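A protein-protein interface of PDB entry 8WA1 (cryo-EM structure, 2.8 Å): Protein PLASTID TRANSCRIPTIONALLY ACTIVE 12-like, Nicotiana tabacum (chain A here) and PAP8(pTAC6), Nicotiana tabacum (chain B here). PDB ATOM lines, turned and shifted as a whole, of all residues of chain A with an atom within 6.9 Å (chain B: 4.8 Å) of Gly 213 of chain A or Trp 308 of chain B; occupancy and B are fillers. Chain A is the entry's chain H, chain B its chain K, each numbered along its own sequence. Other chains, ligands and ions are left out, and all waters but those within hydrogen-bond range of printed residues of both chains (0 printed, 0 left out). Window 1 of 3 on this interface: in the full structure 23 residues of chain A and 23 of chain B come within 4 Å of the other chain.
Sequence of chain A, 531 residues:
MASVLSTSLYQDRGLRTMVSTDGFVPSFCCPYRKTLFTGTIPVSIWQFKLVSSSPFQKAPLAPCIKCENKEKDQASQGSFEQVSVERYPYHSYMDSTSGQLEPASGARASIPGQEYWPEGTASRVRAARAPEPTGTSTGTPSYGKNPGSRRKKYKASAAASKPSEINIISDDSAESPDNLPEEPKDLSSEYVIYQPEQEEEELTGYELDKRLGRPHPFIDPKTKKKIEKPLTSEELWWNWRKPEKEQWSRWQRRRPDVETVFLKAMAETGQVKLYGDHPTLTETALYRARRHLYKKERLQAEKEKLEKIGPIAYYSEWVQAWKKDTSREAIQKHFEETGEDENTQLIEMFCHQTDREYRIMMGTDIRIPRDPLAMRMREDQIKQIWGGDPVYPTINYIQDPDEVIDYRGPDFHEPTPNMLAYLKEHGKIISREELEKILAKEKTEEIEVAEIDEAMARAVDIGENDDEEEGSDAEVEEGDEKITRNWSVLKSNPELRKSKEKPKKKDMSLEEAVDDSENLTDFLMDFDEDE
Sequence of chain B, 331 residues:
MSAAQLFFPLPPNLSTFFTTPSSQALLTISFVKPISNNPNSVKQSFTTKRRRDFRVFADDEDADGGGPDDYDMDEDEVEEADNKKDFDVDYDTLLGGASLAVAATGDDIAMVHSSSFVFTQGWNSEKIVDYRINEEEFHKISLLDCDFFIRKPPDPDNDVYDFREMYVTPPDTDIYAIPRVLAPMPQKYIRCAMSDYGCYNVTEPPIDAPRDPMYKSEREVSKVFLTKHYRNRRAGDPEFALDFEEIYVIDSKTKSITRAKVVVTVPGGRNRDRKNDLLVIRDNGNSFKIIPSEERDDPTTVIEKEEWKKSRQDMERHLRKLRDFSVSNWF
Gly 213 of chain A touches two residues of chain B. Printed residues of chain B within 4 Å of Arg 214 of chain A: Trp 330. Of the printed residues of chain B, Pro 215 of chain A touches Trp 330 (3.2 Å). Of the printed residues of chain B, His 216 of chain A touches Arg 312 and Trp 330. Of chain A, only Gly 213 (3.8 Å) comes within 4 Å of Trp 308 of chain B. Of the printed residues of chain A, Arg 312 of chain B touches His 216. Printed residues of chain A within 4 Å of Trp 330 of chain B: Gly 213 (3.2 Å), Arg 214 (3.5 Å), Pro 215 (3.2 Å), His 216 (2.9 Å) and Arg 290 (3.6 Å). The nearest printed residue of chain B that does not touch Gly 213 of chain A is Arg 312 of chain B (5.7 Å). The nearest residue of chain A that does not touch Trp 308 of chain B is Arg 211 of chain A (4.1 Å).
Among the printed residues, merely in contact across the chains: Pro 215 of chain A with Trp 330 of chain B (3.2 Å), Gly 213 of chain A with Trp 330 of chain B (3.2 Å), Arg 290 of chain A with Trp 330 of chain B (3.6 Å), His 216 of chain A with Arg 312 of chain B (3.6 Å) and Gly 213 of chain A with Trp 308 of chain B (3.8 Å).
The side-chain hydroxyl (OG) of Ser 311 of chain B is in hydrogen-bond range of the backbone carbonyl oxygen (O) of Trp 308 of chain B (2.8 Å). The guanidinium group (NE) of Arg 214 of chain A lies within salt-bridge range of the side-chain carboxylate (OD1) of Asp 209 of chain A (3.3 Å). O of Arg 214 of chain A sits at hydrogen-bond distance from ND1 of His 216 of chain A (2.7 Å).
N of Trp 330 of chain B sits at hydrogen-bond distance from O of His 216 of chain A. The backbone carbonyl oxygen (O) of Arg 214 of chain A sits close to the backbone carbonyl oxygen (O) of Trp 330 of chain B (3.5 Å).
Hydrophobic or aromatic side chains of chain A within 4 Å of the printed part of chain B: His 216. Hydrophobic or aromatic side chains of chain B that line the printed part of chain A: Trp 308 and Trp 330. Among the printed residues, 7 pairs touch across the chains. Among the printed residues, no Asp or Glu carboxylate lies within 4 Å of a Lys or Arg side-chain nitrogen of the other chain.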
ATOM      1  N   GLU A 207     -25.757  -5.430  -7.903  1.00  0.00           N
ATOM      2  CA  GLU A 207     -26.098  -5.699  -9.296  1.00  0.00           C
ATOM      3  C   GLU A 207     -27.544  -5.328  -9.595  1.00  0.00           C
ATOM      4  O   GLU A 207     -27.846  -4.818 -10.679  1.00  0.00           O
ATOM      5  CB  GLU A 207     -25.840  -7.168  -9.627  1.00  0.00           C
ATOM      6  CG  GLU A 207     -24.383  -7.587  -9.503  1.00  0.00           C
ATOM      7  CD  GLU A 207     -23.495  -6.943 -10.551  1.00  0.00           C
ATOM      8  OE1 GLU A 207     -24.016  -6.530 -11.608  1.00  0.00           O
ATOM      9  OE2 GLU A 207     -22.271  -6.850 -10.317  1.00  0.00           O
ATOM     10  N   LEU A 208     -28.450  -5.564  -8.643  1.00  0.00           N
ATOM     11  CA  LEU A 208     -29.848  -5.198  -8.855  1.00  0.00           C
ATOM     12  C   LEU A 208     -30.007  -3.689  -8.993  1.00  0.00           C
ATOM     13  O   LEU A 208     -30.746  -3.212  -9.863  1.00  0.00           O
ATOM     14  CB  LEU A 208     -30.709  -5.726  -7.708  1.00  0.00           C
ATOM     15  CG  LEU A 208     -32.214  -5.483  -7.815  1.00  0.00           C
ATOM     16  CD1 LEU A 208     -32.781  -6.172  -9.046  1.00  0.00           C
ATOM     17  CD2 LEU A 208     -32.921  -5.957  -6.557  1.00  0.00           C
ATOM     18  N   ASP A 209     -29.318  -2.920  -8.146  1.00  0.00           N
ATOM     19  CA  ASP A 209     -29.406  -1.468  -8.233  1.00  0.00           C
ATOM     20  C   ASP A 209     -28.732  -0.947  -9.496  1.00  0.00           C
ATOM     21  O   ASP A 209     -29.190   0.039 -10.086  1.00  0.00           O
ATOM     22  CB  ASP A 209     -28.790  -0.829  -6.989  1.00  0.00           C
ATOM     23  CG  ASP A 209     -29.566  -1.148  -5.728  1.00  0.00           C
ATOM     24  OD1 ASP A 209     -30.576  -1.878  -5.820  1.00  0.00           O
ATOM     25  OD2 ASP A 209     -29.168  -0.667  -4.647  1.00  0.00           O
ATOM     26  N   LYS A 210     -27.648  -1.593  -9.928  1.00  0.00           N
ATOM     27  CA  LYS A 210     -26.998  -1.185 -11.169  1.00  0.00           C
ATOM     28  C   LYS A 210     -27.883  -1.479 -12.373  1.00  0.00           C
ATOM     29  O   LYS A 210     -27.887  -0.722 -13.352  1.00  0.00           O
ATOM     30  CB  LYS A 210     -25.645  -1.883 -11.305  1.00  0.00           C
ATOM     31  CG  LYS A 210     -24.779  -1.353 -12.437  1.00  0.00           C
ATOM     32  CD  LYS A 210     -23.414  -2.024 -12.448  1.00  0.00           C
ATOM     33  CE  LYS A 210     -22.502  -1.403 -13.493  1.00  0.00           C
ATOM     34  NZ  LYS A 210     -23.069  -1.507 -14.866  1.00  0.00           N
ATOM     35  N   ARG A 211     -28.643  -2.574 -12.319  1.00  0.00           N
ATOM     36  CA  ARG A 211     -29.540  -2.906 -13.421  1.00  0.00           C
ATOM     37  C   ARG A 211     -30.752  -1.982 -13.451  1.00  0.00           C
ATOM     38  O   ARG A 211     -31.118  -1.467 -14.513  1.00  0.00           O
ATOM     39  CB  ARG A 211     -29.986  -4.364 -13.321  1.00  0.00           C
ATOM     40  CG  ARG A 211     -28.906  -5.375 -13.674  1.00  0.00           C
ATOM     41  CD  ARG A 211     -29.442  -6.801 -13.644  1.00  0.00           C
ATOM     42  NE  ARG A 211     -30.525  -7.010 -14.602  1.00  0.00           N
ATOM     43  CZ  ARG A 211     -31.815  -7.029 -14.281  1.00  0.00           C
ATOM     44  NH1 ARG A 211     -32.731  -7.226 -15.219  1.00  0.00           N
ATOM     45  NH2 ARG A 211     -32.190  -6.852 -13.021  1.00  0.00           N
ATOM     46  N   LEU A 212     -31.382  -1.756 -12.300  1.00  0.00           N
ATOM     47  CA  LEU A 212     -32.599  -0.958 -12.222  1.00  0.00           C
ATOM     48  C   LEU A 212     -32.325   0.536 -12.117  1.00  0.00           C
ATOM     49  O   LEU A 212     -33.275   1.320 -12.020  1.00  0.00           O
ATOM     50  CB  LEU A 212     -33.451  -1.409 -11.032  1.00  0.00           C
ATOM     51  CG  LEU A 212     -33.958  -2.850 -11.048  1.00  0.00           C
ATOM     52  CD1 LEU A 212     -34.822  -3.122  -9.827  1.00  0.00           C
ATOM     53  CD2 LEU A 212     -34.728  -3.137 -12.328  1.00  0.00           C
ATOM     54  N   GLY A 213     -31.061   0.948 -12.138  1.00  0.00           N
ATOM     55  CA  GLY A 213     -30.724   2.355 -12.047  1.00  0.00           C
ATOM     56  C   GLY A 213     -31.115   2.990 -10.728  1.00  0.00           C
ATOM     57  O   GLY A 213     -31.689   4.083 -10.701  1.00  0.00           O
ATOM     58  N   ARG A 214     -30.809   2.311  -9.627  1.00  0.00           N
ATOM     59  CA  ARG A 214     -31.121   2.793  -8.288  1.00  0.00           C
ATOM     60  C   ARG A 214     -29.857   3.351  -7.643  1.00  0.00           C
ATOM     61  O   ARG A 214     -28.748   3.063  -8.114  1.00  0.00           O
ATOM     62  CB  ARG A 214     -31.724   1.659  -7.451  1.00  0.00           C
ATOM     63  CG  ARG A 214     -33.134   1.272  -7.871  1.00  0.00           C
ATOM     64  CD  ARG A 214     -33.527  -0.099  -7.343  1.00  0.00           C
ATOM     65  NE  ARG A 214     -33.397  -0.195  -5.892  1.00  0.00           N
ATOM     66  CZ  ARG A 214     -33.710  -1.276  -5.187  1.00  0.00           C
ATOM     67  NH1 ARG A 214     -34.175  -2.356  -5.798  1.00  0.00           N
ATOM     68  NH2 ARG A 214     -33.558  -1.278  -3.869  1.00  0.00           N
ATOM     69  N   PRO A 215     -29.970   4.157  -6.586  1.00  0.00           N
ATOM     70  CA  PRO A 215     -28.765   4.710  -5.946  1.00  0.00           C
ATOM     71  C   PRO A 215     -27.844   3.612  -5.438  1.00  0.00           C
ATOM     72  O   PRO A 215     -28.215   2.807  -4.582  1.00  0.00           O
ATOM     73  CB  PRO A 215     -29.335   5.552  -4.798  1.00  0.00           C
ATOM     74  CG  PRO A 215     -30.693   5.937  -5.266  1.00  0.00           C
ATOM     75  CD  PRO A 215     -31.202   4.759  -6.045  1.00  0.00           C
ATOM     76  N   HIS A 216     -26.625   3.584  -5.984  1.00  0.00           N
ATOM     77  CA  HIS A 216     -25.624   2.591  -5.636  1.00  0.00           C
ATOM     78  C   HIS A 216     -24.252   3.177  -5.934  1.00  0.00           C
ATOM     79  O   HIS A 216     -24.125   3.993  -6.857  1.00  0.00           O
ATOM     80  CB  HIS A 216     -25.813   1.288  -6.419  1.00  0.00           C
ATOM     81  CG  HIS A 216     -25.496   1.408  -7.876  1.00  0.00           C
ATOM     82  ND1 HIS A 216     -26.353   2.002  -8.778  1.00  0.00           N
ATOM     83  CD2 HIS A 216     -24.414   1.014  -8.589  1.00  0.00           C
ATOM     84  CE1 HIS A 216     -25.813   1.968  -9.984  1.00  0.00           C
ATOM     85  NE2 HIS A 216     -24.637   1.372  -9.896  1.00  0.00           N
ATOM     86  N   ARG A 290     -29.077  15.102 -14.876  1.00  0.00           N
ATOM     87  CA  ARG A 290     -30.361  14.433 -14.681  1.00  0.00           C
ATOM     88  C   ARG A 290     -31.317  15.185 -13.749  1.00  0.00           C
ATOM     89  O   ARG A 290     -32.214  14.562 -13.170  1.00  0.00           O
ATOM     90  CB  ARG A 290     -30.124  13.017 -14.155  1.00  0.00           C
ATOM     91  CG  ARG A 290     -28.997  12.289 -14.868  1.00  0.00           C
ATOM     92  CD  ARG A 290     -28.684  10.949 -14.226  1.00  0.00           C
ATOM     93  NE  ARG A 290     -29.609   9.900 -14.647  1.00  0.00           N
ATOM     94  CZ  ARG A 290     -30.621   9.455 -13.912  1.00  0.00           C
ATOM     95  NH1 ARG A 290     -31.406   8.496 -14.380  1.00  0.00           N
ATOM     96  NH2 ARG A 290     -30.844   9.961 -12.707  1.00  0.00           N
ATOM     97  N   LEU A 293     -35.401  15.019 -14.337  1.00  0.00           N
ATOM     98  CA  LEU A 293     -36.193  13.903 -13.832  1.00  0.00           C
ATOM     99  C   LEU A 293     -36.708  14.181 -12.427  1.00  0.00           C
ATOM    100  O   LEU A 293     -37.897  13.999 -12.146  1.00  0.00           O
ATOM    101  CB  LEU A 293     -35.359  12.626 -13.852  1.00  0.00           C
ATOM    102  CG  LEU A 293     -34.826  12.234 -15.226  1.00  0.00           C
ATOM    103  CD1 LEU A 293     -33.823  11.103 -15.110  1.00  0.00           C
ATOM    104  CD2 LEU A 293     -35.982  11.842 -16.126  1.00  0.00           C
ATOM    105  N   GLU B 304     -35.969   2.573 -25.880  1.00  0.00           N
ATOM    106  CA  GLU B 304     -35.572   3.251 -24.652  1.00  0.00           C
ATOM    107  C   GLU B 304     -34.596   2.408 -23.846  1.00  0.00           C
ATOM    108  O   GLU B 304     -33.667   2.943 -23.236  1.00  0.00           O
ATOM    109  CB  GLU B 304     -36.806   3.592 -23.816  1.00  0.00           C
ATOM    110  CG  GLU B 304     -37.660   4.709 -24.392  1.00  0.00           C
ATOM    111  CD  GLU B 304     -38.893   4.988 -23.557  1.00  0.00           C
ATOM    112  OE1 GLU B 304     -39.128   4.250 -22.577  1.00  0.00           O
ATOM    113  OE2 GLU B 304     -39.629   5.944 -23.878  1.00  0.00           O
ATOM    114  N   LYS B 305     -34.780   1.085 -23.838  1.00  0.00           N
ATOM    115  CA  LYS B 305     -33.852   0.213 -23.125  1.00  0.00           C
ATOM    116  C   LYS B 305     -32.446   0.314 -23.698  1.00  0.00           C
ATOM    117  O   LYS B 305     -31.472   0.494 -22.953  1.00  0.00           O
ATOM    118  CB  LYS B 305     -34.345  -1.232 -23.178  1.00  0.00           C
ATOM    119  CG  LYS B 305     -35.460  -1.554 -22.198  1.00  0.00           C
ATOM    120  CD  LYS B 305     -36.048  -2.930 -22.467  1.00  0.00           C
ATOM    121  CE  LYS B 305     -34.960  -3.983 -22.621  1.00  0.00           C
ATOM    122  NZ  LYS B 305     -34.076  -4.061 -21.426  1.00  0.00           N
ATOM    123  N   GLU B 306     -32.316   0.200 -25.022  1.00  0.00           N
ATOM    124  CA  GLU B 306     -30.991   0.261 -25.632  1.00  0.00           C
ATOM    125  C   GLU B 306     -30.370   1.643 -25.466  1.00  0.00           C
ATOM    126  O   GLU B 306     -29.169   1.761 -25.183  1.00  0.00           O
ATOM    127  CB  GLU B 306     -31.072  -0.132 -27.106  1.00  0.00           C
ATOM    128  CG  GLU B 306     -29.720  -0.406 -27.745  1.00  0.00           C
ATOM    129  CD  GLU B 306     -29.811  -1.385 -28.897  1.00  0.00           C
ATOM    130  OE1 GLU B 306     -30.905  -1.948 -29.107  1.00  0.00           O
ATOM    131  OE2 GLU B 306     -28.792  -1.595 -29.588  1.00  0.00           O
ATOM    132  N   GLU B 307     -31.171   2.702 -25.632  1.00  0.00           N
ATOM    133  CA  GLU B 307     -30.659   4.052 -25.428  1.00  0.00           C
ATOM    134  C   GLU B 307     -30.183   4.252 -23.996  1.00  0.00           C
ATOM    135  O   GLU B 307     -29.122   4.843 -23.767  1.00  0.00           O
ATOM    136  CB  GLU B 307     -31.732   5.081 -25.786  1.00  0.00           C
ATOM    137  CG  GLU B 307     -31.949   5.267 -27.280  1.00  0.00           C
ATOM    138  CD  GLU B 307     -30.797   5.989 -27.953  1.00  0.00           C
ATOM    139  OE1 GLU B 307     -30.020   6.665 -27.244  1.00  0.00           O
ATOM    140  OE2 GLU B 307     -30.667   5.881 -29.190  1.00  0.00           O
ATOM    141  N   TRP B 308     -30.948   3.759 -23.020  1.00  0.00           N
ATOM    142  CA  TRP B 308     -30.569   3.912 -21.621  1.00  0.00           C
ATOM    143  C   TRP B 308     -29.292   3.145 -21.312  1.00  0.00           C
ATOM    144  O   TRP B 308     -28.422   3.643 -20.591  1.00  0.00           O
ATOM    145  CB  TRP B 308     -31.712   3.445 -20.720  1.00  0.00           C
ATOM    146  CG  TRP B 308     -31.581   3.876 -19.293  1.00  0.00           C
ATOM    147  CD1 TRP B 308     -32.056   5.028 -18.737  1.00  0.00           C
ATOM    148  CD2 TRP B 308     -30.937   3.156 -18.234  1.00  0.00           C
ATOM    149  NE1 TRP B 308     -31.747   5.072 -17.400  1.00  0.00           N
ATOM    150  CE2 TRP B 308     -31.060   3.935 -17.066  1.00  0.00           C
ATOM    151  CE3 TRP B 308     -30.270   1.931 -18.160  1.00  0.00           C
ATOM    152  CZ2 TRP B 308     -30.539   3.528 -15.840  1.00  0.00           C
ATOM    153  CZ3 TRP B 308     -29.753   1.529 -16.942  1.00  0.00           C
ATOM    154  CH2 TRP B 308     -29.891   2.325 -15.798  1.00  0.00           C
ATOM    155  N   LYS B 309     -29.158   1.933 -21.857  1.00  0.00           N
ATOM    156  CA  LYS B 309     -27.937   1.163 -21.635  1.00  0.00           C
ATOM    157  C   LYS B 309     -26.721   1.876 -22.217  1.00  0.00           C
ATOM    158  O   LYS B 309     -25.692   2.025 -21.539  1.00  0.00           O
ATOM    159  CB  LYS B 309     -28.081  -0.234 -22.237  1.00  0.00           C
ATOM    160  CG  LYS B 309     -26.836  -1.097 -22.112  1.00  0.00           C
ATOM    161  CD  LYS B 309     -27.066  -2.485 -22.686  1.00  0.00           C
ATOM    162  CE  LYS B 309     -27.449  -2.421 -24.156  1.00  0.00           C
ATOM    163  NZ  LYS B 309     -26.389  -1.776 -24.979  1.00  0.00           N
ATOM    164  N   LYS B 310     -26.819   2.328 -23.471  1.00  0.00           N
ATOM    165  CA  LYS B 310     -25.690   3.018 -24.090  1.00  0.00           C
ATOM    166  C   LYS B 310     -25.355   4.307 -23.350  1.00  0.00           C
ATOM    167  O   LYS B 310     -24.176   4.632 -23.159  1.00  0.00           O
ATOM    168  CB  LYS B 310     -25.986   3.304 -25.561  1.00  0.00           C
ATOM    169  CG  LYS B 310     -26.126   2.061 -26.423  1.00  0.00           C
ATOM    170  CD  LYS B 310     -26.109   2.409 -27.904  1.00  0.00           C
ATOM    171  CE  LYS B 310     -27.226   3.377 -28.263  1.00  0.00           C
ATOM    172  NZ  LYS B 310     -28.570   2.801 -27.984  1.00  0.00           N
ATOM    173  N   SER B 311     -26.376   5.048 -22.911  1.00  0.00           N
ATOM    174  CA  SER B 311     -26.133   6.297 -22.201  1.00  0.00           C
ATOM    175  C   SER B 311     -25.485   6.046 -20.848  1.00  0.00           C
ATOM    176  O   SER B 311     -24.588   6.788 -20.439  1.00  0.00           O
ATOM    177  CB  SER B 311     -27.440   7.067 -22.033  1.00  0.00           C
ATOM    178  OG  SER B 311     -28.375   6.314 -21.283  1.00  0.00           O
ATOM    179  N   ARG B 312     -25.922   5.002 -20.138  1.00  0.00           N
ATOM    180  CA  ARG B 312     -25.294   4.662 -18.866  1.00  0.00           C
ATOM    181  C   ARG B 312     -23.831   4.291 -19.060  1.00  0.00           C
ATOM    182  O   ARG B 312     -22.960   4.749 -18.309  1.00  0.00           O
ATOM    183  CB  ARG B 312     -26.051   3.516 -18.196  1.00  0.00           C
ATOM    184  CG  ARG B 312     -26.927   3.943 -17.033  1.00  0.00           C
ATOM    185  CD  ARG B 312     -26.427   3.354 -15.725  1.00  0.00           C
ATOM    186  NE  ARG B 312     -25.028   3.684 -15.478  1.00  0.00           N
ATOM    187  CZ  ARG B 312     -24.349   3.300 -14.402  1.00  0.00           C
ATOM    188  NH1 ARG B 312     -24.943   2.571 -13.467  1.00  0.00           N
ATOM    189  NH2 ARG B 312     -23.077   3.645 -14.259  1.00  0.00           N
ATOM    190  N   TRP B 330     -23.992   6.659  -7.938  1.00  0.00           N
ATOM    191  CA  TRP B 330     -24.859   6.940  -9.073  1.00  0.00           C
ATOM    192  C   TRP B 330     -26.308   6.998  -8.609  1.00  0.00           C
ATOM    193  O   TRP B 330     -26.865   5.993  -8.160  1.00  0.00           O
ATOM    194  CB  TRP B 330     -24.694   5.876 -10.157  1.00  0.00           C
ATOM    195  CG  TRP B 330     -25.334   6.245 -11.464  1.00  0.00           C
ATOM    196  CD1 TRP B 330     -24.733   6.856 -12.526  1.00  0.00           C
ATOM    197  CD2 TRP B 330     -26.698   6.030 -11.845  1.00  0.00           C
ATOM    198  NE1 TRP B 330     -25.636   7.034 -13.545  1.00  0.00           N
ATOM    199  CE2 TRP B 330     -26.851   6.535 -13.151  1.00  0.00           C
ATOM    200  CE3 TRP B 330     -27.804   5.459 -11.210  1.00  0.00           C
ATOM    201  CZ2 TRP B 330     -28.064   6.488 -13.834  1.00  0.00           C
ATOM    202  CZ3 TRP B 330     -29.007   5.414 -11.887  1.00  0.00           C
ATOM    203  CH2 TRP B 330     -29.128   5.924 -13.186  1.00  0.00           C
